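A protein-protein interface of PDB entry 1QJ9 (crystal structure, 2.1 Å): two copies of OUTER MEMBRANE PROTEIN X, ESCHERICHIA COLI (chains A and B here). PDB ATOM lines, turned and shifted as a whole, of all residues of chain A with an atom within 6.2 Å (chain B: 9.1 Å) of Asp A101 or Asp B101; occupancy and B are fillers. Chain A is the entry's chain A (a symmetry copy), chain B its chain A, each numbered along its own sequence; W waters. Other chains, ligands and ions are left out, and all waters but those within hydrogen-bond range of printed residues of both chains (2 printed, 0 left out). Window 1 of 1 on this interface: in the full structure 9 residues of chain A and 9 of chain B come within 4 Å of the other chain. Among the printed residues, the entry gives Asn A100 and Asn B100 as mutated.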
ATOM      1  N   LYS A  89      -4.823  -8.507  26.674  1.00  0.00           N
ATOM      2  CA  LYS A  89      -3.428  -8.019  26.632  1.00  0.00           C
ATOM      3  C   LYS A  89      -2.509  -9.243  26.637  1.00  0.00           C
ATOM      4  O   LYS A  89      -2.504 -10.040  27.596  1.00  0.00           O
ATOM      5  CB  LYS A  89      -3.176  -7.066  27.786  1.00  0.00           C
ATOM      6  CG  LYS A  89      -1.810  -6.323  27.785  1.00  0.00           C
ATOM      7  CD  LYS A  89      -1.642  -5.545  29.072  1.00  0.00           C
ATOM      8  CE  LYS A  89      -0.309  -4.865  29.286  1.00  0.00           C
ATOM      9  NZ  LYS A  89      -0.121  -3.615  28.492  1.00  0.00           N
ATOM     10  N   PHE A  90      -1.791  -9.440  25.533  1.00  0.00           N
ATOM     11  CA  PHE A  90      -0.844 -10.527  25.386  1.00  0.00           C
ATOM     12  C   PHE A  90       0.618  -9.988  25.467  1.00  0.00           C
ATOM     13  O   PHE A  90       1.002  -9.079  24.718  1.00  0.00           O
ATOM     14  CB  PHE A  90      -1.003 -11.254  24.043  1.00  0.00           C
ATOM     15  CG  PHE A  90      -0.047 -12.422  23.835  1.00  0.00           C
ATOM     16  CD1 PHE A  90       0.318 -13.272  24.868  1.00  0.00           C
ATOM     17  CD2 PHE A  90       0.446 -12.718  22.567  1.00  0.00           C
ATOM     18  CE1 PHE A  90       1.175 -14.338  24.685  1.00  0.00           C
ATOM     19  CE2 PHE A  90       1.303 -13.789  22.352  1.00  0.00           C
ATOM     20  CZ  PHE A  90       1.672 -14.608  23.406  1.00  0.00           C
ATOM     21  N   GLN A  91       1.381 -10.506  26.401  1.00  0.00           N
ATOM     22  CA  GLN A  91       2.761 -10.199  26.646  1.00  0.00           C
ATOM     23  C   GLN A  91       3.621 -11.438  26.310  1.00  0.00           C
ATOM     24  O   GLN A  91       3.253 -12.551  26.693  1.00  0.00           O
ATOM     25  CB  GLN A  91       3.066  -9.841  28.117  1.00  0.00           C
ATOM     26  CG  GLN A  91       2.424  -8.555  28.595  1.00  0.00           C
ATOM     27  CD  GLN A  91       2.770  -8.173  30.017  1.00  0.00           C
ATOM     28  OE1 GLN A  91       3.728  -7.425  30.296  1.00  0.00           O
ATOM     29  NE2 GLN A  91       1.994  -8.647  30.973  1.00  0.00           N
ATOM     30  N   THR A  92       4.751 -11.229  25.641  1.00  0.00           N
ATOM     31  CA  THR A  92       5.675 -12.314  25.299  1.00  0.00           C
ATOM     32  C   THR A  92       7.127 -11.835  25.380  1.00  0.00           C
ATOM     33  O   THR A  92       7.427 -10.731  24.934  1.00  0.00           O
ATOM     34  CB  THR A  92       5.412 -12.907  23.915  1.00  0.00           C
ATOM     35  OG1 THR A  92       6.221 -14.099  23.768  1.00  0.00           O
ATOM     36  CG2 THR A  92       5.746 -11.939  22.792  1.00  0.00           C
ATOM     37  N   THR A  93       7.944 -12.513  26.168  1.00  0.00           N
ATOM     38  CA  THR A  93       9.334 -12.202  26.324  1.00  0.00           C
ATOM     39  C   THR A  93      10.124 -13.420  25.777  1.00  0.00           C
ATOM     40  O   THR A  93      10.071 -14.494  26.346  1.00  0.00           O
ATOM     41  CB  THR A  93       9.796 -11.885  27.738  1.00  0.00           C
ATOM     42  OG1 THR A  93       9.810 -13.067  28.563  1.00  0.00           O
ATOM     43  CG2 THR A  93       8.902 -10.848  28.385  1.00  0.00           C
ATOM     44  N   LYS A  99      11.006  -8.485  23.974  1.00  0.00           N
ATOM     45  CA  LYS A  99       9.717  -8.260  24.626  1.00  0.00           C
ATOM     46  C   LYS A  99       8.760  -7.740  23.545  1.00  0.00           C
ATOM     47  O   LYS A  99       9.161  -6.910  22.697  1.00  0.00           O
ATOM     48  CB  LYS A  99       9.768  -7.300  25.787  1.00  0.00           C
ATOM     49  CG  LYS A  99      10.438  -7.588  27.071  1.00  0.00           C
ATOM     50  CD  LYS A  99      11.887  -7.710  27.277  1.00  0.00           C
ATOM     51  CE  LYS A  99      12.852  -6.565  27.374  1.00  0.00           C
ATOM     52  NZ  LYS A  99      13.337  -5.932  26.116  1.00  0.00           N
ATOM     53  N   ASN A 100       7.577  -8.355  23.460  1.00  0.00           N
ATOM     54  CA  ASN A 100       6.575  -7.904  22.476  1.00  0.00           C
ATOM     55  C   ASN A 100       5.198  -8.007  23.162  1.00  0.00           C
ATOM     56  O   ASN A 100       4.831  -8.992  23.808  1.00  0.00           O
ATOM     57  CB  ASN A 100       6.643  -8.675  21.207  1.00  0.00           C
ATOM     58  CG  ASN A 100       5.772  -8.259  20.068  1.00  0.00           C
ATOM     59  OD1 ASN A 100       5.911  -8.831  18.966  1.00  0.00           O
ATOM     60  ND2 ASN A 100       4.899  -7.295  20.222  1.00  0.00           N
ATOM     61  N   ASP A 101       4.492  -6.883  23.185  1.00  0.00           N
ATOM     62  CA  ASP A 101       3.249  -6.707  23.868  1.00  0.00           C
ATOM     63  C   ASP A 101       2.193  -6.140  22.910  1.00  0.00           C
ATOM     64  O   ASP A 101       2.412  -5.145  22.229  1.00  0.00           O
ATOM     65  CB  ASP A 101       3.355  -5.771  25.061  1.00  0.00           C
ATOM     66  CG  ASP A 101       4.327  -6.168  26.146  1.00  0.00           C
ATOM     67  OD1 ASP A 101       4.815  -7.329  26.158  1.00  0.00           O
ATOM     68  OD2 ASP A 101       4.601  -5.298  27.024  1.00  0.00           O
ATOM     69  N   THR A 102       1.031  -6.829  22.950  1.00  0.00           N
ATOM     70  CA  THR A 102      -0.042  -6.337  22.070  1.00  0.00           C
ATOM     71  C   THR A 102      -1.376  -6.313  22.785  1.00  0.00           C
ATOM     72  O   THR A 102      -1.646  -7.072  23.716  1.00  0.00           O
ATOM     73  CB  THR A 102       0.001  -7.122  20.768  1.00  0.00           C
ATOM     74  OG1 THR A 102      -0.975  -6.555  19.883  1.00  0.00           O
ATOM     75  CG2 THR A 102      -0.270  -8.600  20.946  1.00  0.00           C
ATOM     76  N   SER A 103      -2.192  -5.302  22.497  1.00  0.00           N
ATOM     77  CA  SER A 103      -3.495  -5.213  23.179  1.00  0.00           C
ATOM     78  C   SER A 103      -4.536  -4.673  22.211  1.00  0.00           C
ATOM     79  O   SER A 103      -4.173  -4.101  21.178  1.00  0.00           O
ATOM     80  CB  SER A 103      -3.383  -4.403  24.440  1.00  0.00           C
ATOM     81  OG  SER A 103      -3.158  -3.015  24.230  1.00  0.00           O
ATOM     82  N   TYR B  57      -0.503   6.061  15.337  1.00  0.00           N
ATOM     83  CA  TYR B  57       0.590   6.632  16.084  1.00  0.00           C
ATOM     84  C   TYR B  57       1.710   5.598  16.266  1.00  0.00           C
ATOM     85  O   TYR B  57       1.475   4.376  16.344  1.00  0.00           O
ATOM     86  CB  TYR B  57       0.117   7.164  17.421  1.00  0.00           C
ATOM     87  CG  TYR B  57       1.130   7.383  18.513  1.00  0.00           C
ATOM     88  CD1 TYR B  57       1.609   6.315  19.271  1.00  0.00           C
ATOM     89  CD2 TYR B  57       1.594   8.655  18.830  1.00  0.00           C
ATOM     90  CE1 TYR B  57       2.518   6.506  20.290  1.00  0.00           C
ATOM     91  CE2 TYR B  57       2.492   8.865  19.854  1.00  0.00           C
ATOM     92  CZ  TYR B  57       2.959   7.782  20.583  1.00  0.00           C
ATOM     93  OH  TYR B  57       3.862   7.977  21.607  1.00  0.00           O
ATOM     94  N   ASN B  58       2.948   6.113  16.162  1.00  0.00           N
ATOM     95  CA  ASN B  58       4.122   5.287  16.393  1.00  0.00           C
ATOM     96  C   ASN B  58       5.230   6.088  17.087  1.00  0.00           C
ATOM     97  O   ASN B  58       5.367   7.291  16.883  1.00  0.00           O
ATOM     98  CB  ASN B  58       4.617   4.386  15.340  1.00  0.00           C
ATOM     99  CG  ASN B  58       4.250   4.279  13.926  1.00  0.00           C
ATOM    100  OD1 ASN B  58       4.671   3.306  13.257  1.00  0.00           O
ATOM    101  ND2 ASN B  58       3.461   5.175  13.339  1.00  0.00           N
ATOM    102  N   LYS B  59       5.906   5.402  18.000  1.00  0.00           N
ATOM    103  CA  LYS B  59       6.970   6.049  18.770  1.00  0.00           C
ATOM    104  C   LYS B  59       8.150   5.075  18.932  1.00  0.00           C
ATOM    105  O   LYS B  59       7.944   3.962  19.350  1.00  0.00           O
ATOM    106  CB  LYS B  59       6.473   6.492  20.125  1.00  0.00           C
ATOM    107  CG  LYS B  59       7.462   7.220  20.989  1.00  0.00           C
ATOM    108  CD  LYS B  59       6.873   7.477  22.377  1.00  0.00           C
ATOM    109  CE  LYS B  59       7.863   8.380  23.121  1.00  0.00           C
ATOM    110  NZ  LYS B  59       7.388   8.642  24.500  1.00  0.00           N
ATOM    111  N   GLN B  61      12.126   4.834  20.447  1.00  0.00           N
ATOM    112  CA  GLN B  61      13.130   5.354  21.362  1.00  0.00           C
ATOM    113  C   GLN B  61      14.403   4.501  21.249  1.00  0.00           C
ATOM    114  O   GLN B  61      14.269   3.288  21.081  1.00  0.00           O
ATOM    115  CB  GLN B  61      12.605   5.320  22.794  1.00  0.00           C
ATOM    116  CG  GLN B  61      11.463   6.332  23.018  1.00  0.00           C
ATOM    117  CD  GLN B  61      10.891   5.980  24.407  1.00  0.00           C
ATOM    118  OE1 GLN B  61      10.410   4.848  24.530  1.00  0.00           O
ATOM    119  NE2 GLN B  61      10.983   6.888  25.333  1.00  0.00           N
ATOM    120  N   TYR B  87      19.638  -0.262  23.140  1.00  0.00           N
ATOM    121  CA  TYR B  87      18.269  -0.705  23.485  1.00  0.00           C
ATOM    122  C   TYR B  87      17.278   0.092  22.640  1.00  0.00           C
ATOM    123  O   TYR B  87      17.419   1.309  22.584  1.00  0.00           O
ATOM    124  CB  TYR B  87      17.982  -0.381  24.944  1.00  0.00           C
ATOM    125  CG  TYR B  87      16.525  -0.579  25.352  1.00  0.00           C
ATOM    126  CD1 TYR B  87      16.054  -1.857  25.643  1.00  0.00           C
ATOM    127  CD2 TYR B  87      15.652   0.481  25.461  1.00  0.00           C
ATOM    128  CE1 TYR B  87      14.750  -2.077  26.038  1.00  0.00           C
ATOM    129  CE2 TYR B  87      14.345   0.296  25.884  1.00  0.00           C
ATOM    130  CZ  TYR B  87      13.896  -0.989  26.161  1.00  0.00           C
ATOM    131  OH  TYR B  87      12.597  -1.206  26.544  1.00  0.00           O
ATOM    132  N   GLY B  88      16.339  -0.594  21.988  1.00  0.00           N
ATOM    133  CA  GLY B  88      15.358   0.152  21.188  1.00  0.00           C
ATOM    134  C   GLY B  88      13.930  -0.230  21.624  1.00  0.00           C
ATOM    135  O   GLY B  88      13.665  -1.389  21.952  1.00  0.00           O
ATOM    136  N   LYS B  89      13.021   0.736  21.653  1.00  0.00           N
ATOM    137  CA  LYS B  89      11.621   0.434  22.024  1.00  0.00           C
ATOM    138  C   LYS B  89      10.716   1.058  20.959  1.00  0.00           C
ATOM    139  O   LYS B  89      10.701   2.290  20.769  1.00  0.00           O
ATOM    140  CB  LYS B  89      11.338   0.932  23.429  1.00  0.00           C
ATOM    141  CG  LYS B  89       9.965   0.535  24.041  1.00  0.00           C
ATOM    142  CD  LYS B  89       9.766   1.238  25.367  1.00  0.00           C
ATOM    143  CE  LYS B  89       8.421   1.058  26.035  1.00  0.00           C
ATOM    144  NZ  LYS B  89       8.235  -0.267  26.697  1.00  0.00           N
ATOM    145  N   PHE B  90      10.020   0.205  20.210  1.00  0.00           N
ATOM    146  CA  PHE B  90       9.087   0.627  19.185  1.00  0.00           C
ATOM    147  C   PHE B  90       7.619   0.405  19.662  1.00  0.00           C
ATOM    148  O   PHE B  90       7.239  -0.709  20.049  1.00  0.00           O
ATOM    149  CB  PHE B  90       9.278  -0.150  17.875  1.00  0.00           C
ATOM    150  CG  PHE B  90       8.339   0.262  16.748  1.00  0.00           C
ATOM    151  CD1 PHE B  90       7.964   1.581  16.543  1.00  0.00           C
ATOM    152  CD2 PHE B  90       7.873  -0.679  15.834  1.00  0.00           C
ATOM    153  CE1 PHE B  90       7.121   1.963  15.518  1.00  0.00           C
ATOM    154  CE2 PHE B  90       7.030  -0.322  14.789  1.00  0.00           C
ATOM    155  CZ  PHE B  90       6.651   0.999  14.621  1.00  0.00           C
ATOM    156  N   GLN B  91       6.844   1.464  19.683  1.00  0.00           N
ATOM    157  CA  GLN B  91       5.456   1.502  20.047  1.00  0.00           C
ATOM    158  C   GLN B  91       4.616   1.842  18.796  1.00  0.00           C
ATOM    159  O   GLN B  91       4.988   2.746  18.044  1.00  0.00           O
ATOM    160  CB  GLN B  91       5.121   2.577  21.104  1.00  0.00           C
ATOM    161  CG  GLN B  91       5.740   2.333  22.465  1.00  0.00           C
ATOM    162  CD  GLN B  91       5.364   3.353  23.516  1.00  0.00           C
ATOM    163  OE1 GLN B  91       4.394   3.198  24.283  1.00  0.00           O
ATOM    164  NE2 GLN B  91       6.127   4.425  23.615  1.00  0.00           N
ATOM    165  N   THR B  92       3.496   1.149  18.611  1.00  0.00           N
ATOM    166  CA  THR B  92       2.591   1.403  17.487  1.00  0.00           C
ATOM    167  C   THR B  92       1.132   1.211  17.912  1.00  0.00           C
ATOM    168  O   THR B  92       0.829   0.258  18.625  1.00  0.00           O
ATOM    169  CB  THR B  92       2.885   0.523  16.273  1.00  0.00           C
ATOM    170  OG1 THR B  92       2.091   1.001  15.160  1.00  0.00           O
ATOM    171  CG2 THR B  92       2.562  -0.941  16.520  1.00  0.00           C
ATOM    172  N   THR B  93       0.308   2.226  17.721  1.00  0.00           N
ATOM    173  CA  THR B  93      -1.088   2.187  18.042  1.00  0.00           C
ATOM    174  C   THR B  93      -1.855   2.334  16.702  1.00  0.00           C
ATOM    175  O   THR B  93      -1.802   3.375  16.074  1.00  0.00           O
ATOM    176  CB  THR B  93      -1.580   3.231  19.032  1.00  0.00           C
ATOM    177  OG1 THR B  93      -1.596   4.546  18.441  1.00  0.00           O
ATOM    178  CG2 THR B  93      -0.708   3.263  20.270  1.00  0.00           C
ATOM    179  N   GLU B  94      -2.477   1.226  16.326  1.00  0.00           N
ATOM    180  CA  GLU B  94      -3.253   1.131  15.095  1.00  0.00           C
ATOM    181  C   GLU B  94      -4.730   1.387  15.374  1.00  0.00           C
ATOM    182  O   GLU B  94      -5.406   0.615  16.057  1.00  0.00           O
ATOM    183  CB  GLU B  94      -3.016  -0.240  14.496  1.00  0.00           C
ATOM    184  CG  GLU B  94      -3.798  -0.598  13.252  1.00  0.00           C
ATOM    185  CD  GLU B  94      -3.485  -2.028  12.811  1.00  0.00           C
ATOM    186  OE1 GLU B  94      -2.293  -2.313  12.543  1.00  0.00           O
ATOM    187  OE2 GLU B  94      -4.445  -2.831  12.800  1.00  0.00           O
ATOM    188  N   TYR B  98      -5.772  -0.737  18.622  1.00  0.00           N
ATOM    189  CA  TYR B  98      -4.798  -1.823  18.663  1.00  0.00           C
ATOM    190  C   TYR B  98      -3.454  -1.157  19.067  1.00  0.00           C
ATOM    191  O   TYR B  98      -3.194   0.001  18.704  1.00  0.00           O
ATOM    192  CB  TYR B  98      -4.793  -2.534  17.330  1.00  0.00           C
ATOM    193  CG  TYR B  98      -3.596  -3.424  17.113  1.00  0.00           C
ATOM    194  CD1 TYR B  98      -2.394  -2.867  16.642  1.00  0.00           C
ATOM    195  CD2 TYR B  98      -3.629  -4.763  17.434  1.00  0.00           C
ATOM    196  CE1 TYR B  98      -1.263  -3.666  16.465  1.00  0.00           C
ATOM    197  CE2 TYR B  98      -2.525  -5.570  17.244  1.00  0.00           C
ATOM    198  CZ  TYR B  98      -1.355  -5.006  16.742  1.00  0.00           C
ATOM    199  OH  TYR B  98      -0.241  -5.806  16.580  1.00  0.00           O
ATOM    200  N   LYS B  99      -2.756  -1.757  19.993  1.00  0.00           N
ATOM    201  CA  LYS B  99      -1.481  -1.299  20.544  1.00  0.00           C
ATOM    202  C   LYS B  99      -0.510  -2.484  20.453  1.00  0.00           C
ATOM    203  O   LYS B  99      -0.904  -3.643  20.722  1.00  0.00           O
ATOM    204  CB  LYS B  99      -1.563  -0.797  21.964  1.00  0.00           C
ATOM    205  CG  LYS B  99      -2.254   0.445  22.364  1.00  0.00           C
ATOM    206  CD  LYS B  99      -3.705   0.669  22.338  1.00  0.00           C
ATOM    207  CE  LYS B  99      -4.684   0.154  23.352  1.00  0.00           C
ATOM    208  NZ  LYS B  99      -5.152  -1.255  23.241  1.00  0.00           N
ATOM    209  N   ASN B 100       0.681  -2.229  19.903  1.00  0.00           N
ATOM    210  CA  ASN B 100       1.696  -3.294  19.804  1.00  0.00           C
ATOM    211  C   ASN B 100       3.062  -2.638  20.093  1.00  0.00           C
ATOM    212  O   ASN B 100       3.426  -1.575  19.587  1.00  0.00           O
ATOM    213  CB  ASN B 100       1.660  -3.987  18.490  1.00  0.00           C
ATOM    214  CG  ASN B 100       2.547  -5.169  18.277  1.00  0.00           C
ATOM    215  OD1 ASN B 100       2.434  -5.822  17.218  1.00  0.00           O
ATOM    216  ND2 ASN B 100       3.408  -5.523  19.200  1.00  0.00           N
ATOM    217  N   ASP B 101       3.755  -3.188  21.082  1.00  0.00           N
ATOM    218  CA  ASP B 101       4.983  -2.681  21.607  1.00  0.00           C
ATOM    219  C   ASP B 101       6.051  -3.782  21.620  1.00  0.00           C
ATOM    220  O   ASP B 101       5.835  -4.880  22.121  1.00  0.00           O
ATOM    221  CB  ASP B 101       4.846  -2.139  23.021  1.00  0.00           C
ATOM    222  CG  ASP B 101       3.858  -1.014  23.219  1.00  0.00           C
ATOM    223  OD1 ASP B 101       3.382  -0.413  22.221  1.00  0.00           O
ATOM    224  OD2 ASP B 101       3.559  -0.711  24.412  1.00  0.00           O
ATOM    225  N   THR B 102       7.219  -3.382  21.072  1.00  0.00           N
ATOM    226  CA  THR B 102       8.303  -4.378  21.061  1.00  0.00           C
ATOM    227  C   THR B 102       9.623  -3.763  21.474  1.00  0.00           C
ATOM    228  O   THR B 102       9.884  -2.572  21.306  1.00  0.00           O
ATOM    229  CB  THR B 102       8.292  -5.092  19.719  1.00  0.00           C
ATOM    230  OG1 THR B 102       9.278  -6.133  19.769  1.00  0.00           O
ATOM    231  CG2 THR B 102       8.575  -4.178  18.548  1.00  0.00           C
ATOM    232  N   SER B 103      10.434  -4.522  22.208  1.00  0.00           N
ATOM    233  CA  SER B 103      11.723  -3.969  22.658  1.00  0.00           C
ATOM    234  C   SER B 103      12.776  -5.065  22.644  1.00  0.00           C
ATOM    235  O   SER B 103      12.426  -6.249  22.597  1.00  0.00           O
ATOM    236  CB  SER B 103      11.579  -3.304  24.000  1.00  0.00           C
ATOM    237  OG  SER B 103      11.344  -4.200  25.078  1.00  0.00           O
ATOM    238  N   ASP B 104      14.060  -4.684  22.457  1.00  0.00           N
ATOM    239  CA  ASP B 104      15.110  -5.688  22.492  1.00  0.00           C
ATOM    240  C   ASP B 104      16.451  -4.962  22.729  1.00  0.00           C
ATOM    241  O   ASP B 104      16.467  -3.761  22.542  1.00  0.00           O
ATOM    242  CB  ASP B 104      15.206  -6.468  21.191  1.00  0.00           C
ATOM    243  CG  ASP B 104      15.829  -7.838  21.436  1.00  0.00           C
ATOM    244  OD1 ASP B 104      16.396  -8.141  22.518  1.00  0.00           O
ATOM    245  OD2 ASP B 104      15.683  -8.690  20.551  1.00  0.00           O
HETATM  246  O   HOH W   1      12.277  -3.726  28.317  1.00  0.00           O
HETATM  247  O   HOH W   2      -4.155  -0.489  26.282  1.00  0.00           O
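Water W1 lies within hydrogen-bond range of the side-chain hydroxyl of Tyr B87, the side-chain amino group of Lys A99 and the side-chain hydroxyl of Ser B103. Water W2 lies within hydrogen-bond range of the side-chain amino group (NZ) of Lys B99 (3.3 Å) and the side-chain hydroxyl (OG) of Ser A103 (3.4 Å).
Asp B101 touches Lys A99 (O to O, 3.9 Å). NZ of Lys A99 touches N of Asp B104 (3.9 Å). CB of Asn A100 touches OG1 of Thr B102, 3.9 Å away. Lys B99 touches Asp A101. CB of Asn B100 touches OG1 of Thr A102, at 3.9 Å. Tyr B98 touches Ser A103 (CA to O, 3.5 Å).
Printed residues of chain B that touch a printed residue of chain A: Tyr B98, Lys B99, Asn B100, Asp B101, Thr B102, Ser B103 and Asp B104. Hydrophobic or aromatic side chains of chain B within 4 Å of the printed part of chain A: Tyr B98. Among the printed residues, 15 pairs touch across the chains.
Lys A99 touches Asp B101, and with the chains exchanged Asp A101 touches Lys B99. Asn A100 touches its own counterpart, Asn B100. Asn A100 touches Asp B101, and with the chains exchanged Asp A101 touches Asn B100. Asn A100 touches Thr B102, and with the chains exchanged Thr A102 touches Asn B100. Of the 15 pairs that touch across the chains among the printed residues, 12 have their exchanged pair printed and touching as well.
Of chain B, only Asn B100, Asp B101 and Thr B102 come within 4 Å of Asn A100. Of chain B, only Lys B99, Asn B100 and Asp B101 come within 4 Å of Asp A101. Printed residues of chain A within 4 Å of Tyr B98: Thr A102 (3.2 Å) and Ser A103 (3.5 Å). Of the printed residues of chain A, Thr B102 touches Lys A99 (3.0 Å) and Asn A100 (3.9 Å). The nearest residue of chain B that does not touch Asp A101 is Thr B102 (4.9 Å). The nearest residue of chain A that does not touch Asp B101 is Thr A102 (4.9 Å). The nearest printed residue of chain B that does not touch Ser A103 is Asn B100 (4.9 Å).
OD1 of Asn B100 is in hydrogen-bond range of OH of Tyr B98 (2.8 Å). The backbone carbonyl oxygen of Asp B104 sits at hydrogen-bond distance from the backbone NH of Gly B88, at 3.2 Å. The backbone NH of Asn A100 is in hydrogen-bond range of the backbone carbonyl oxygen of Thr A92, 2.8 Å away. The backbone carbonyl oxygen (O) of Thr B92 lies within hydrogen-bond range of the backbone NH (N) of Asn B100 (2.8 Å). O of Phe A90 is in hydrogen-bond range of N of Thr A102 (2.9 Å). The backbone carbonyl oxygen (O) of Phe B90 is in hydrogen-bond range of the backbone NH (N) of Thr B102 (2.9 Å).
The backbone carbonyl oxygen (O) of Lys A99 lies within hydrogen-bond range of the side-chain hydroxyl (OG1) of Thr B102, 3.0 Å away. ND2 of Asn B100 lies close to ND2 of Asn A100 (2.5 Å). The side-chain amide nitrogen (ND2) of Asn B100 sits close to the backbone carbonyl oxygen (O) of Asp A101. O of Asp A101 lies within hydrogen-bond range of N of Asp B101. The side-chain hydroxyl (OG1) of Thr A102 is in hydrogen-bond range of the backbone carbonyl oxygen (O) of Lys B99 (3.0 Å). The backbone carbonyl oxygen (O) of Asp B101 sits close to the side-chain amide nitrogen (ND2) of Asn A100 (3.2 Å). The backbone NH (N) of Ser B103 lies within hydrogen-bond range of the backbone carbonyl oxygen (O) of Lys A99, 2.7 Å away. O of Lys B99 is in hydrogen-bond range of N of Ser A103 (2.7 Å). The side-chain hydroxyl (OH) of Tyr B98 sits close to the side-chain hydroxyl (OG1) of Thr A102 (3.5 Å).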
